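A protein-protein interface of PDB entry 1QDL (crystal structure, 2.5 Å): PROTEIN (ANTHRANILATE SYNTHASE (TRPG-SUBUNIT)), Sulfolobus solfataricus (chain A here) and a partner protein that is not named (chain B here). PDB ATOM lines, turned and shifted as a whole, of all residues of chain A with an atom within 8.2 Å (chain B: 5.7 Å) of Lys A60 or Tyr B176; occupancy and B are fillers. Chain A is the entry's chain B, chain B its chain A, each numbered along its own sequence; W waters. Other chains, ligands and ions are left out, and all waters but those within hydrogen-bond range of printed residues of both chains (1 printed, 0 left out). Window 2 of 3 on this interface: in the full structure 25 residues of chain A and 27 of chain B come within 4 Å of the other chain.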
ATOM      1  N   TYR A  10     -28.650  -1.069   2.149  1.00  0.00           N
ATOM      2  CA  TYR A  10     -29.609  -0.180   2.806  1.00  0.00           C
ATOM      3  C   TYR A  10     -29.402   1.261   2.367  1.00  0.00           C
ATOM      4  O   TYR A  10     -29.321   2.180   3.179  1.00  0.00           O
ATOM      5  CB  TYR A  10     -29.469  -0.310   4.311  1.00  0.00           C
ATOM      6  CG  TYR A  10     -29.913  -1.664   4.797  1.00  0.00           C
ATOM      7  CD1 TYR A  10     -29.078  -2.782   4.676  1.00  0.00           C
ATOM      8  CD2 TYR A  10     -31.176  -1.836   5.362  1.00  0.00           C
ATOM      9  CE1 TYR A  10     -29.496  -4.041   5.111  1.00  0.00           C
ATOM     10  CE2 TYR A  10     -31.603  -3.084   5.798  1.00  0.00           C
ATOM     11  CZ  TYR A  10     -30.763  -4.183   5.673  1.00  0.00           C
ATOM     12  OH  TYR A  10     -31.201  -5.412   6.112  1.00  0.00           O
ATOM     13  N   ASN A  33     -27.787  -6.550   1.202  1.00  0.00           N
ATOM     14  CA  ASN A  33     -26.611  -7.283   1.643  1.00  0.00           C
ATOM     15  C   ASN A  33     -26.841  -8.429   2.628  1.00  0.00           C
ATOM     16  O   ASN A  33     -25.963  -9.268   2.814  1.00  0.00           O
ATOM     17  CB  ASN A  33     -25.577  -6.303   2.211  1.00  0.00           C
ATOM     18  CG  ASN A  33     -25.992  -5.702   3.551  1.00  0.00           C
ATOM     19  OD1 ASN A  33     -26.616  -6.358   4.393  1.00  0.00           O
ATOM     20  ND2 ASN A  33     -25.630  -4.442   3.756  1.00  0.00           N
ATOM     21  N   GLY A  54     -23.622   2.881   0.491  1.00  0.00           N
ATOM     22  CA  GLY A  54     -24.241   2.574   1.760  1.00  0.00           C
ATOM     23  C   GLY A  54     -23.506   3.169   2.936  1.00  0.00           C
ATOM     24  O   GLY A  54     -22.344   3.597   2.819  1.00  0.00           O
ATOM     25  N   PRO A  55     -24.188   3.233   4.088  1.00  0.00           N
ATOM     26  CA  PRO A  55     -23.614   3.776   5.316  1.00  0.00           C
ATOM     27  C   PRO A  55     -22.642   2.779   5.925  1.00  0.00           C
ATOM     28  O   PRO A  55     -22.815   1.561   5.798  1.00  0.00           O
ATOM     29  CB  PRO A  55     -24.830   4.007   6.209  1.00  0.00           C
ATOM     30  CG  PRO A  55     -25.814   3.011   5.759  1.00  0.00           C
ATOM     31  CD  PRO A  55     -25.584   2.804   4.284  1.00  0.00           C
ATOM     32  N   GLY A  56     -21.607   3.299   6.564  1.00  0.00           N
ATOM     33  CA  GLY A  56     -20.655   2.420   7.194  1.00  0.00           C
ATOM     34  C   GLY A  56     -19.376   2.179   6.434  1.00  0.00           C
ATOM     35  O   GLY A  56     -19.065   2.864   5.447  1.00  0.00           O
ATOM     36  N   THR A  57     -18.650   1.172   6.920  1.00  0.00           N
ATOM     37  CA  THR A  57     -17.354   0.757   6.393  1.00  0.00           C
ATOM     38  C   THR A  57     -17.372  -0.725   6.063  1.00  0.00           C
ATOM     39  O   THR A  57     -18.130  -1.484   6.661  1.00  0.00           O
ATOM     40  CB  THR A  57     -16.251   0.991   7.454  1.00  0.00           C
ATOM     41  OG1 THR A  57     -15.090   0.214   7.133  1.00  0.00           O
ATOM     42  CG2 THR A  57     -16.759   0.581   8.838  1.00  0.00           C
ATOM     43  N   PRO A  58     -16.529  -1.158   5.107  1.00  0.00           N
ATOM     44  CA  PRO A  58     -16.497  -2.581   4.755  1.00  0.00           C
ATOM     45  C   PRO A  58     -15.799  -3.343   5.872  1.00  0.00           C
ATOM     46  O   PRO A  58     -15.924  -4.559   5.974  1.00  0.00           O
ATOM     47  CB  PRO A  58     -15.699  -2.638   3.453  1.00  0.00           C
ATOM     48  CG  PRO A  58     -15.203  -1.249   3.192  1.00  0.00           C
ATOM     49  CD  PRO A  58     -15.559  -0.362   4.336  1.00  0.00           C
ATOM     50  N   GLU A  59     -15.064  -2.607   6.705  1.00  0.00           N
ATOM     51  CA  GLU A  59     -14.335  -3.180   7.827  1.00  0.00           C
ATOM     52  C   GLU A  59     -15.294  -3.859   8.801  1.00  0.00           C
ATOM     53  O   GLU A  59     -14.889  -4.739   9.555  1.00  0.00           O
ATOM     54  CB  GLU A  59     -13.541  -2.092   8.554  1.00  0.00           C
ATOM     55  CG  GLU A  59     -12.427  -1.470   7.731  1.00  0.00           C
ATOM     56  CD  GLU A  59     -11.518  -0.577   8.565  1.00  0.00           C
ATOM     57  OE1 GLU A  59     -11.722  -0.498   9.796  1.00  0.00           O
ATOM     58  OE2 GLU A  59     -10.596   0.044   7.991  1.00  0.00           O
ATOM     59  N   LYS A  60     -16.561  -3.444   8.788  1.00  0.00           N
ATOM     60  CA  LYS A  60     -17.587  -4.034   9.655  1.00  0.00           C
ATOM     61  C   LYS A  60     -18.541  -4.840   8.777  1.00  0.00           C
ATOM     62  O   LYS A  60     -19.182  -4.283   7.893  1.00  0.00           O
ATOM     63  CB  LYS A  60     -18.376  -2.942  10.384  1.00  0.00           C
ATOM     64  CG  LYS A  60     -17.528  -2.028  11.238  1.00  0.00           C
ATOM     65  CD  LYS A  60     -18.341  -1.439  12.369  1.00  0.00           C
ATOM     66  CE  LYS A  60     -17.493  -0.504  13.216  1.00  0.00           C
ATOM     67  NZ  LYS A  60     -18.165   0.804  13.464  1.00  0.00           N
ATOM     68  N   ARG A  61     -18.650  -6.143   9.024  1.00  0.00           N
ATOM     69  CA  ARG A  61     -19.510  -6.989   8.203  1.00  0.00           C
ATOM     70  C   ARG A  61     -20.988  -6.620   8.160  1.00  0.00           C
ATOM     71  O   ARG A  61     -21.622  -6.744   7.112  1.00  0.00           O
ATOM     72  CB  ARG A  61     -19.368  -8.457   8.604  1.00  0.00           C
ATOM     73  CG  ARG A  61     -19.513  -9.415   7.418  1.00  0.00           C
ATOM     74  CD  ARG A  61     -20.105 -10.754   7.847  1.00  0.00           C
ATOM     75  NE  ARG A  61     -21.218 -11.182   7.001  1.00  0.00           N
ATOM     76  CZ  ARG A  61     -21.075 -11.704   5.788  1.00  0.00           C
ATOM     77  NH1 ARG A  61     -19.860 -11.861   5.275  1.00  0.00           N
ATOM     78  NH2 ARG A  61     -22.144 -12.077   5.095  1.00  0.00           N
ATOM     79  N   GLU A  62     -21.548  -6.176   9.278  1.00  0.00           N
ATOM     80  CA  GLU A  62     -22.958  -5.804   9.278  1.00  0.00           C
ATOM     81  C   GLU A  62     -23.223  -4.648   8.311  1.00  0.00           C
ATOM     82  O   GLU A  62     -24.353  -4.442   7.867  1.00  0.00           O
ATOM     83  CB  GLU A  62     -23.404  -5.414  10.679  1.00  0.00           C
ATOM     84  CG  GLU A  62     -22.263  -5.158  11.633  1.00  0.00           C
ATOM     85  CD  GLU A  62     -22.655  -4.206  12.747  1.00  0.00           C
ATOM     86  OE1 GLU A  62     -21.877  -3.263  13.022  1.00  0.00           O
ATOM     87  OE2 GLU A  62     -23.742  -4.403  13.344  1.00  0.00           O
ATOM     88  N   ASP A  63     -22.171  -3.903   7.986  1.00  0.00           N
ATOM     89  CA  ASP A  63     -22.270  -2.774   7.069  1.00  0.00           C
ATOM     90  C   ASP A  63     -22.355  -3.227   5.606  1.00  0.00           C
ATOM     91  O   ASP A  63     -23.121  -2.662   4.821  1.00  0.00           O
ATOM     92  CB  ASP A  63     -21.059  -1.849   7.239  1.00  0.00           C
ATOM     93  CG  ASP A  63     -21.133  -1.007   8.498  1.00  0.00           C
ATOM     94  OD1 ASP A  63     -22.107  -1.147   9.274  1.00  0.00           O
ATOM     95  OD2 ASP A  63     -20.208  -0.200   8.711  1.00  0.00           O
ATOM     96  N   ILE A  64     -21.578  -4.245   5.243  1.00  0.00           N
ATOM     97  CA  ILE A  64     -21.575  -4.730   3.872  1.00  0.00           C
ATOM     98  C   ILE A  64     -22.266  -6.075   3.638  1.00  0.00           C
ATOM     99  O   ILE A  64     -22.566  -6.421   2.495  1.00  0.00           O
ATOM    100  CB  ILE A  64     -20.149  -4.838   3.340  1.00  0.00           C
ATOM    101  CG1 ILE A  64     -19.276  -5.536   4.374  1.00  0.00           C
ATOM    102  CG2 ILE A  64     -19.609  -3.469   3.025  1.00  0.00           C
ATOM    103  CD1 ILE A  64     -19.011  -6.973   4.035  1.00  0.00           C
ATOM    104  N   GLY A  65     -22.522  -6.829   4.704  1.00  0.00           N
ATOM    105  CA  GLY A  65     -23.175  -8.123   4.551  1.00  0.00           C
ATOM    106  C   GLY A  65     -22.431  -9.085   3.631  1.00  0.00           C
ATOM    107  O   GLY A  65     -21.209  -9.254   3.736  1.00  0.00           O
ATOM    108  N   LEU A  68     -18.668  -8.680   0.659  1.00  0.00           N
ATOM    109  CA  LEU A  68     -17.252  -9.019   0.533  1.00  0.00           C
ATOM    110  C   LEU A  68     -16.936 -10.402  -0.023  1.00  0.00           C
ATOM    111  O   LEU A  68     -15.900 -10.600  -0.663  1.00  0.00           O
ATOM    112  CB  LEU A  68     -16.554  -8.823   1.870  1.00  0.00           C
ATOM    113  CG  LEU A  68     -16.066  -7.383   2.032  1.00  0.00           C
ATOM    114  CD1 LEU A  68     -15.805  -7.104   3.495  1.00  0.00           C
ATOM    115  CD2 LEU A  68     -14.806  -7.159   1.206  1.00  0.00           C
ATOM    116  N   LEU A  85     -19.599   2.640  -0.803  1.00  0.00           N
ATOM    117  CA  LEU A  85     -19.330   1.508   0.084  1.00  0.00           C
ATOM    118  C   LEU A  85     -18.820   0.307  -0.737  1.00  0.00           C
ATOM    119  O   LEU A  85     -17.879  -0.372  -0.331  1.00  0.00           O
ATOM    120  CB  LEU A  85     -20.608   1.119   0.840  1.00  0.00           C
ATOM    121  CG  LEU A  85     -20.533   0.045   1.932  1.00  0.00           C
ATOM    122  CD1 LEU A  85     -19.472   0.426   2.958  1.00  0.00           C
ATOM    123  CD2 LEU A  85     -21.899  -0.116   2.596  1.00  0.00           C
ATOM    124  N   TYR A  92     -11.110  -2.961   0.137  1.00  0.00           N
ATOM    125  CA  TYR A  92     -10.847  -3.660   1.382  1.00  0.00           C
ATOM    126  C   TYR A  92     -10.616  -5.129   1.058  1.00  0.00           C
ATOM    127  O   TYR A  92      -9.667  -5.736   1.540  1.00  0.00           O
ATOM    128  CB  TYR A  92     -12.052  -3.513   2.311  1.00  0.00           C
ATOM    129  CG  TYR A  92     -11.847  -4.027   3.714  1.00  0.00           C
ATOM    130  CD1 TYR A  92     -10.956  -3.406   4.586  1.00  0.00           C
ATOM    131  CD2 TYR A  92     -12.585  -5.106   4.190  1.00  0.00           C
ATOM    132  CE1 TYR A  92     -10.807  -3.844   5.906  1.00  0.00           C
ATOM    133  CE2 TYR A  92     -12.444  -5.553   5.506  1.00  0.00           C
ATOM    134  CZ  TYR A  92     -11.557  -4.918   6.358  1.00  0.00           C
ATOM    135  OH  TYR A  92     -11.435  -5.354   7.657  1.00  0.00           O
ATOM    136  N   ILE A  98      -8.822   1.329   4.669  1.00  0.00           N
ATOM    137  CA  ILE A  98      -9.978   2.213   4.695  1.00  0.00           C
ATOM    138  C   ILE A  98      -9.703   3.299   5.735  1.00  0.00           C
ATOM    139  O   ILE A  98      -9.364   2.997   6.881  1.00  0.00           O
ATOM    140  CB  ILE A  98     -11.268   1.448   5.101  1.00  0.00           C
ATOM    141  CG1 ILE A  98     -11.610   0.384   4.057  1.00  0.00           C
ATOM    142  CG2 ILE A  98     -12.424   2.413   5.241  1.00  0.00           C
ATOM    143  CD1 ILE A  98     -11.877   0.933   2.673  1.00  0.00           C
ATOM    144  N   ARG A 100     -10.562   7.792   6.895  1.00  0.00           N
ATOM    145  CA  ARG A 100     -11.390   8.970   6.694  1.00  0.00           C
ATOM    146  C   ARG A 100     -10.699   9.779   5.602  1.00  0.00           C
ATOM    147  O   ARG A 100      -9.476   9.682   5.413  1.00  0.00           O
ATOM    148  CB  ARG A 100     -11.499   9.797   7.981  1.00  0.00           C
ATOM    149  CG  ARG A 100     -12.529   9.257   8.947  1.00  0.00           C
ATOM    150  CD  ARG A 100     -13.189  10.327   9.798  1.00  0.00           C
ATOM    151  NE  ARG A 100     -14.007   9.694  10.831  1.00  0.00           N
ATOM    152  CZ  ARG A 100     -14.387  10.273  11.969  1.00  0.00           C
ATOM    153  NH1 ARG A 100     -14.025  11.521  12.241  1.00  0.00           N
ATOM    154  NH2 ARG A 100     -15.119   9.593  12.845  1.00  0.00           N
ATOM    155  N   HIS A 106     -20.023  15.601   0.745  1.00  0.00           N
ATOM    156  CA  HIS A 106     -21.338  15.041   0.946  1.00  0.00           C
ATOM    157  C   HIS A 106     -22.268  15.784   0.014  1.00  0.00           C
ATOM    158  O   HIS A 106     -22.817  16.821   0.376  1.00  0.00           O
ATOM    159  CB  HIS A 106     -21.777  15.236   2.393  1.00  0.00           C
ATOM    160  CG  HIS A 106     -21.195  14.236   3.340  1.00  0.00           C
ATOM    161  ND1 HIS A 106     -20.415  13.182   2.919  1.00  0.00           N
ATOM    162  CD2 HIS A 106     -21.276  14.132   4.687  1.00  0.00           C
ATOM    163  CE1 HIS A 106     -20.040  12.471   3.967  1.00  0.00           C
ATOM    164  NE2 HIS A 106     -20.550  13.026   5.051  1.00  0.00           N
ATOM    165  N   SER A 137     -17.424  10.110   3.576  1.00  0.00           N
ATOM    166  CA  SER A 137     -16.516  10.647   4.580  1.00  0.00           C
ATOM    167  C   SER A 137     -15.251   9.805   4.555  1.00  0.00           C
ATOM    168  O   SER A 137     -14.183  10.261   4.956  1.00  0.00           O
ATOM    169  CB  SER A 137     -17.124  10.583   5.989  1.00  0.00           C
ATOM    170  OG  SER A 137     -18.539  10.498   5.967  1.00  0.00           O
ATOM    171  N   LEU A 138     -15.366   8.570   4.078  1.00  0.00           N
ATOM    172  CA  LEU A 138     -14.198   7.701   4.035  1.00  0.00           C
ATOM    173  C   LEU A 138     -13.708   7.414   2.634  1.00  0.00           C
ATOM    174  O   LEU A 138     -14.444   7.541   1.652  1.00  0.00           O
ATOM    175  CB  LEU A 138     -14.485   6.382   4.752  1.00  0.00           C
ATOM    176  CG  LEU A 138     -15.363   6.498   6.000  1.00  0.00           C
ATOM    177  CD1 LEU A 138     -15.914   5.142   6.358  1.00  0.00           C
ATOM    178  CD2 LEU A 138     -14.560   7.061   7.152  1.00  0.00           C
ATOM    179  N   TYR B 171     -22.015   9.800  14.152  1.00  0.00           N
ATOM    180  CA  TYR B 171     -22.503   8.934  13.088  1.00  0.00           C
ATOM    181  C   TYR B 171     -22.157   9.536  11.738  1.00  0.00           C
ATOM    182  O   TYR B 171     -21.746   8.831  10.819  1.00  0.00           O
ATOM    183  CB  TYR B 171     -24.011   8.797  13.167  1.00  0.00           C
ATOM    184  CG  TYR B 171     -24.509   8.064  14.374  1.00  0.00           C
ATOM    185  CD1 TYR B 171     -24.874   8.755  15.518  1.00  0.00           C
ATOM    186  CD2 TYR B 171     -24.708   6.689  14.343  1.00  0.00           C
ATOM    187  CE1 TYR B 171     -25.441   8.096  16.609  1.00  0.00           C
ATOM    188  CE2 TYR B 171     -25.275   6.015  15.426  1.00  0.00           C
ATOM    189  CZ  TYR B 171     -25.642   6.726  16.556  1.00  0.00           C
ATOM    190  OH  TYR B 171     -26.238   6.077  17.618  1.00  0.00           O
ATOM    191  N   ILE B 172     -22.329  10.847  11.618  1.00  0.00           N
ATOM    192  CA  ILE B 172     -22.040  11.515  10.367  1.00  0.00           C
ATOM    193  C   ILE B 172     -20.559  11.462  10.047  1.00  0.00           C
ATOM    194  O   ILE B 172     -20.179  11.202   8.904  1.00  0.00           O
ATOM    195  CB  ILE B 172     -22.506  12.974  10.399  1.00  0.00           C
ATOM    196  CG1 ILE B 172     -23.993  13.029  10.764  1.00  0.00           C
ATOM    197  CG2 ILE B 172     -22.256  13.616   9.055  1.00  0.00           C
ATOM    198  CD1 ILE B 172     -24.621  14.387  10.583  1.00  0.00           C
ATOM    199  N   ARG B 173     -19.728  11.695  11.061  1.00  0.00           N
ATOM    200  CA  ARG B 173     -18.273  11.676  10.900  1.00  0.00           C
ATOM    201  C   ARG B 173     -17.799  10.278  10.524  1.00  0.00           C
ATOM    202  O   ARG B 173     -16.922  10.113   9.670  1.00  0.00           O
ATOM    203  CB  ARG B 173     -17.591  12.097  12.200  1.00  0.00           C
ATOM    204  CG  ARG B 173     -17.340  13.589  12.324  1.00  0.00           C
ATOM    205  CD  ARG B 173     -18.045  14.166  13.546  1.00  0.00           C
ATOM    206  NE  ARG B 173     -17.125  14.423  14.650  1.00  0.00           N
ATOM    207  CZ  ARG B 173     -17.312  15.367  15.567  1.00  0.00           C
ATOM    208  NH1 ARG B 173     -18.389  16.141  15.506  1.00  0.00           N
ATOM    209  NH2 ARG B 173     -16.422  15.539  16.541  1.00  0.00           N
ATOM    210  N   SER B 174     -18.385   9.281  11.185  1.00  0.00           N
ATOM    211  CA  SER B 174     -18.058   7.881  10.952  1.00  0.00           C
ATOM    212  C   SER B 174     -18.495   7.437   9.567  1.00  0.00           C
ATOM    213  O   SER B 174     -17.921   6.515   8.994  1.00  0.00           O
ATOM    214  CB  SER B 174     -18.738   7.010  11.999  1.00  0.00           C
ATOM    215  OG  SER B 174     -18.569   7.568  13.288  1.00  0.00           O
ATOM    216  N   GLY B 175     -19.521   8.089   9.033  1.00  0.00           N
ATOM    217  CA  GLY B 175     -20.000   7.747   7.709  1.00  0.00           C
ATOM    218  C   GLY B 175     -21.268   6.918   7.702  1.00  0.00           C
ATOM    219  O   GLY B 175     -21.469   6.121   6.783  1.00  0.00           O
ATOM    220  N   TYR B 176     -22.119   7.115   8.710  1.00  0.00           N
ATOM    221  CA  TYR B 176     -23.380   6.381   8.823  1.00  0.00           C
ATOM    222  C   TYR B 176     -24.609   7.184   8.400  1.00  0.00           C
ATOM    223  O   TYR B 176     -25.729   6.669   8.372  1.00  0.00           O
ATOM    224  CB  TYR B 176     -23.536   5.842  10.243  1.00  0.00           C
ATOM    225  CG  TYR B 176     -22.641   4.646  10.458  1.00  0.00           C
ATOM    226  CD1 TYR B 176     -21.404   4.779  11.094  1.00  0.00           C
ATOM    227  CD2 TYR B 176     -22.985   3.398   9.944  1.00  0.00           C
ATOM    228  CE1 TYR B 176     -20.528   3.700  11.202  1.00  0.00           C
ATOM    229  CE2 TYR B 176     -22.117   2.311  10.048  1.00  0.00           C
ATOM    230  CZ  TYR B 176     -20.891   2.471  10.675  1.00  0.00           C
ATOM    231  OH  TYR B 176     -20.024   1.404  10.756  1.00  0.00           O
ATOM    232  N   ILE B 177     -24.380   8.450   8.071  1.00  0.00           N
ATOM    233  CA  ILE B 177     -25.421   9.348   7.587  1.00  0.00           C
ATOM    234  C   ILE B 177     -24.751  10.588   7.013  1.00  0.00           C
ATOM    235  O   ILE B 177     -23.604  10.908   7.336  1.00  0.00           O
ATOM    236  CB  ILE B 177     -26.421   9.794   8.695  1.00  0.00           C
ATOM    237  CG1 ILE B 177     -25.755   9.783  10.070  1.00  0.00           C
ATOM    238  CG2 ILE B 177     -27.652   8.904   8.671  1.00  0.00           C
ATOM    239  CD1 ILE B 177     -26.512  10.596  11.101  1.00  0.00           C
ATOM    240  N   PHE B 178     -25.464  11.260   6.125  1.00  0.00           N
ATOM    241  CA  PHE B 178     -24.970  12.479   5.522  1.00  0.00           C
ATOM    242  C   PHE B 178     -25.692  13.573   6.276  1.00  0.00           C
ATOM    243  O   PHE B 178     -25.117  14.591   6.654  1.00  0.00           O
ATOM    244  CB  PHE B 178     -25.350  12.535   4.047  1.00  0.00           C
ATOM    245  CG  PHE B 178     -24.768  11.429   3.238  1.00  0.00           C
ATOM    246  CD1 PHE B 178     -25.590  10.590   2.496  1.00  0.00           C
ATOM    247  CD2 PHE B 178     -23.389  11.214   3.222  1.00  0.00           C
ATOM    248  CE1 PHE B 178     -25.053   9.548   1.748  1.00  0.00           C
ATOM    249  CE2 PHE B 178     -22.837  10.174   2.476  1.00  0.00           C
ATOM    250  CZ  PHE B 178     -23.671   9.337   1.738  1.00  0.00           C
ATOM    251  N   ALA B 338     -30.431  11.002   5.255  1.00  0.00           N
ATOM    252  CA  ALA B 338     -29.856  10.148   4.227  1.00  0.00           C
ATOM    253  C   ALA B 338     -28.524   9.566   4.658  1.00  0.00           C
ATOM    254  O   ALA B 338     -27.685  10.272   5.222  1.00  0.00           O
ATOM    255  CB  ALA B 338     -29.681  10.930   2.952  1.00  0.00           C
ATOM    256  N   PRO B 339     -28.325   8.253   4.464  1.00  0.00           N
ATOM    257  CA  PRO B 339     -29.247   7.262   3.883  1.00  0.00           C
ATOM    258  C   PRO B 339     -30.490   7.150   4.762  1.00  0.00           C
ATOM    259  O   PRO B 339     -30.385   6.980   5.978  1.00  0.00           O
ATOM    260  CB  PRO B 339     -28.453   5.958   3.879  1.00  0.00           C
ATOM    261  CG  PRO B 339     -27.071   6.300   4.244  1.00  0.00           C
ATOM    262  CD  PRO B 339     -26.999   7.689   4.769  1.00  0.00           C
ATOM    263  N   MET B 342     -30.979   4.250   7.705  1.00  0.00           N
ATOM    264  CA  MET B 342     -30.112   4.505   8.843  1.00  0.00           C
ATOM    265  C   MET B 342     -30.628   5.697   9.626  1.00  0.00           C
ATOM    266  O   MET B 342     -30.858   5.616  10.836  1.00  0.00           O
ATOM    267  CB  MET B 342     -28.695   4.800   8.374  1.00  0.00           C
ATOM    268  CG  MET B 342     -27.712   4.952   9.519  1.00  0.00           C
ATOM    269  SD  MET B 342     -27.568   3.435  10.461  1.00  0.00           S
ATOM    270  CE  MET B 342     -27.156   4.073  12.061  1.00  0.00           C
ATOM    271  N   ALA B 343     -30.803   6.803   8.909  1.00  0.00           N
ATOM    272  CA  ALA B 343     -31.278   8.047   9.488  1.00  0.00           C
ATOM    273  C   ALA B 343     -32.524   7.872  10.345  1.00  0.00           C
ATOM    274  O   ALA B 343     -32.625   8.450  11.424  1.00  0.00           O
ATOM    275  CB  ALA B 343     -31.544   9.064   8.383  1.00  0.00           C
ATOM    276  N   ILE B 346     -31.515   6.062  13.480  1.00  0.00           N
ATOM    277  CA  ILE B 346     -30.750   6.919  14.368  1.00  0.00           C
ATOM    278  C   ILE B 346     -31.738   7.864  15.053  1.00  0.00           C
ATOM    279  O   ILE B 346     -31.591   8.185  16.224  1.00  0.00           O
ATOM    280  CB  ILE B 346     -29.723   7.757  13.610  1.00  0.00           C
ATOM    281  CG1 ILE B 346     -28.500   6.903  13.292  1.00  0.00           C
ATOM    282  CG2 ILE B 346     -29.324   8.963  14.449  1.00  0.00           C
ATOM    283  CD1 ILE B 346     -27.504   7.588  12.377  1.00  0.00           C
HETATM  284  O   HOH W   1     -29.393   3.094   5.844  1.00  0.00           O
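The backbone carbonyl oxygen (O) of Arg B173 sits at hydrogen-bond distance from the guanidinium group (NE) of Arg A100, at 3.2 Å.
The backbone carbonyl oxygen of Gly B175 is in hydrogen-bond range of the backbone NH of Gly A56, 2.8 Å away.
OD2 of Asp A63 sits at hydrogen-bond distance from OH of Tyr B176.
OH of Tyr B176 lies within hydrogen-bond range of NZ of Lys A60, 3.3 Å away.
The side-chain hydroxyl (OG) of Ser A137 is in hydrogen-bond range of the backbone carbonyl oxygen (O) of Ile B172 (3.4 Å).
The backbone carbonyl oxygen (O) of Tyr B171 lies within hydrogen-bond range of the backbone NH (N) of Tyr B176, 2.7 Å away.
The side-chain carboxylate of Asp A63 is in hydrogen-bond range of the backbone NH of Thr A57, 2.7 Å away.
O of Asp A63 lies within hydrogen-bond range of ND2 of Asn A33, 3.3 Å away.
NE2 of His A106 sits close to OG of Ser A137, at 3.4 Å.
The backbone carbonyl oxygen (O) of Ala B338 sits at hydrogen-bond distance from the backbone NH (N) of Phe B178 (2.6 Å).
OG1 of Thr A57 sits at hydrogen-bond distance from N of Glu A59 (2.9 Å).
Among the printed residues, merely in contact across the chains: Tyr A10 with Pro B339 (3.9 Å), Pro A55 with Gly B175 (3.5 Å), Pro A55 with Tyr B176 (3.5 Å), Pro A55 with Pro B339 (3.8 Å), Gly A56 with Tyr B176 (3.2 Å), Thr A57 with Tyr B176 (3.9 Å), Arg A100 with Ser B174 (3.7 Å), His A106 with Phe B178 (3.6 Å), Ser A137 with Arg B173 (3.7 Å), Ser A137 with Gly B175 (3.6 Å) and Leu A138 with Ser B174 (3.6 Å).
Of chain A, only Pro A55, Gly A56, Thr A57, Lys A60 and Asp A63 come within 4 Å of Tyr B176.
Of chain A, only Pro A55, Gly A56 and Ser A137 come within 4 Å of Gly B175.
Of the printed residues of chain A, Arg B173 touches Arg A100 and Ser A137.
Printed residues of chain B within 4 Å of His A106: Phe B178 (3.6 Å).
Of the printed residues of chain B, Asp A63 touches Tyr B176.
Of the printed residues of chain B, Arg A100 touches Arg B173 and Ser B174.
Gly A65 touches none of the printed residues of chain B.
The nearest printed residue of chain A that does not touch Phe B178 is Ser A137 (5.5 Å).
Of the 13 printed residues of chain B, 7 touch a printed residue of chain A.
Hydrophobic or aromatic side chains of chain B that line the printed part of chain A: Tyr B176, Phe B178 and Pro B339.
Among the printed residues, 16 pairs touch across the chains.
Among the printed residues, no Asp or Glu carboxylate lies within 4 Å of a Lys or Arg side-chain nitrogen of the other chain.
Water W1 bridges the backbone NH (N) of Met B342 (2.7 Å) and the backbone carbonyl oxygen (O) of Tyr A10 (2.8 Å).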
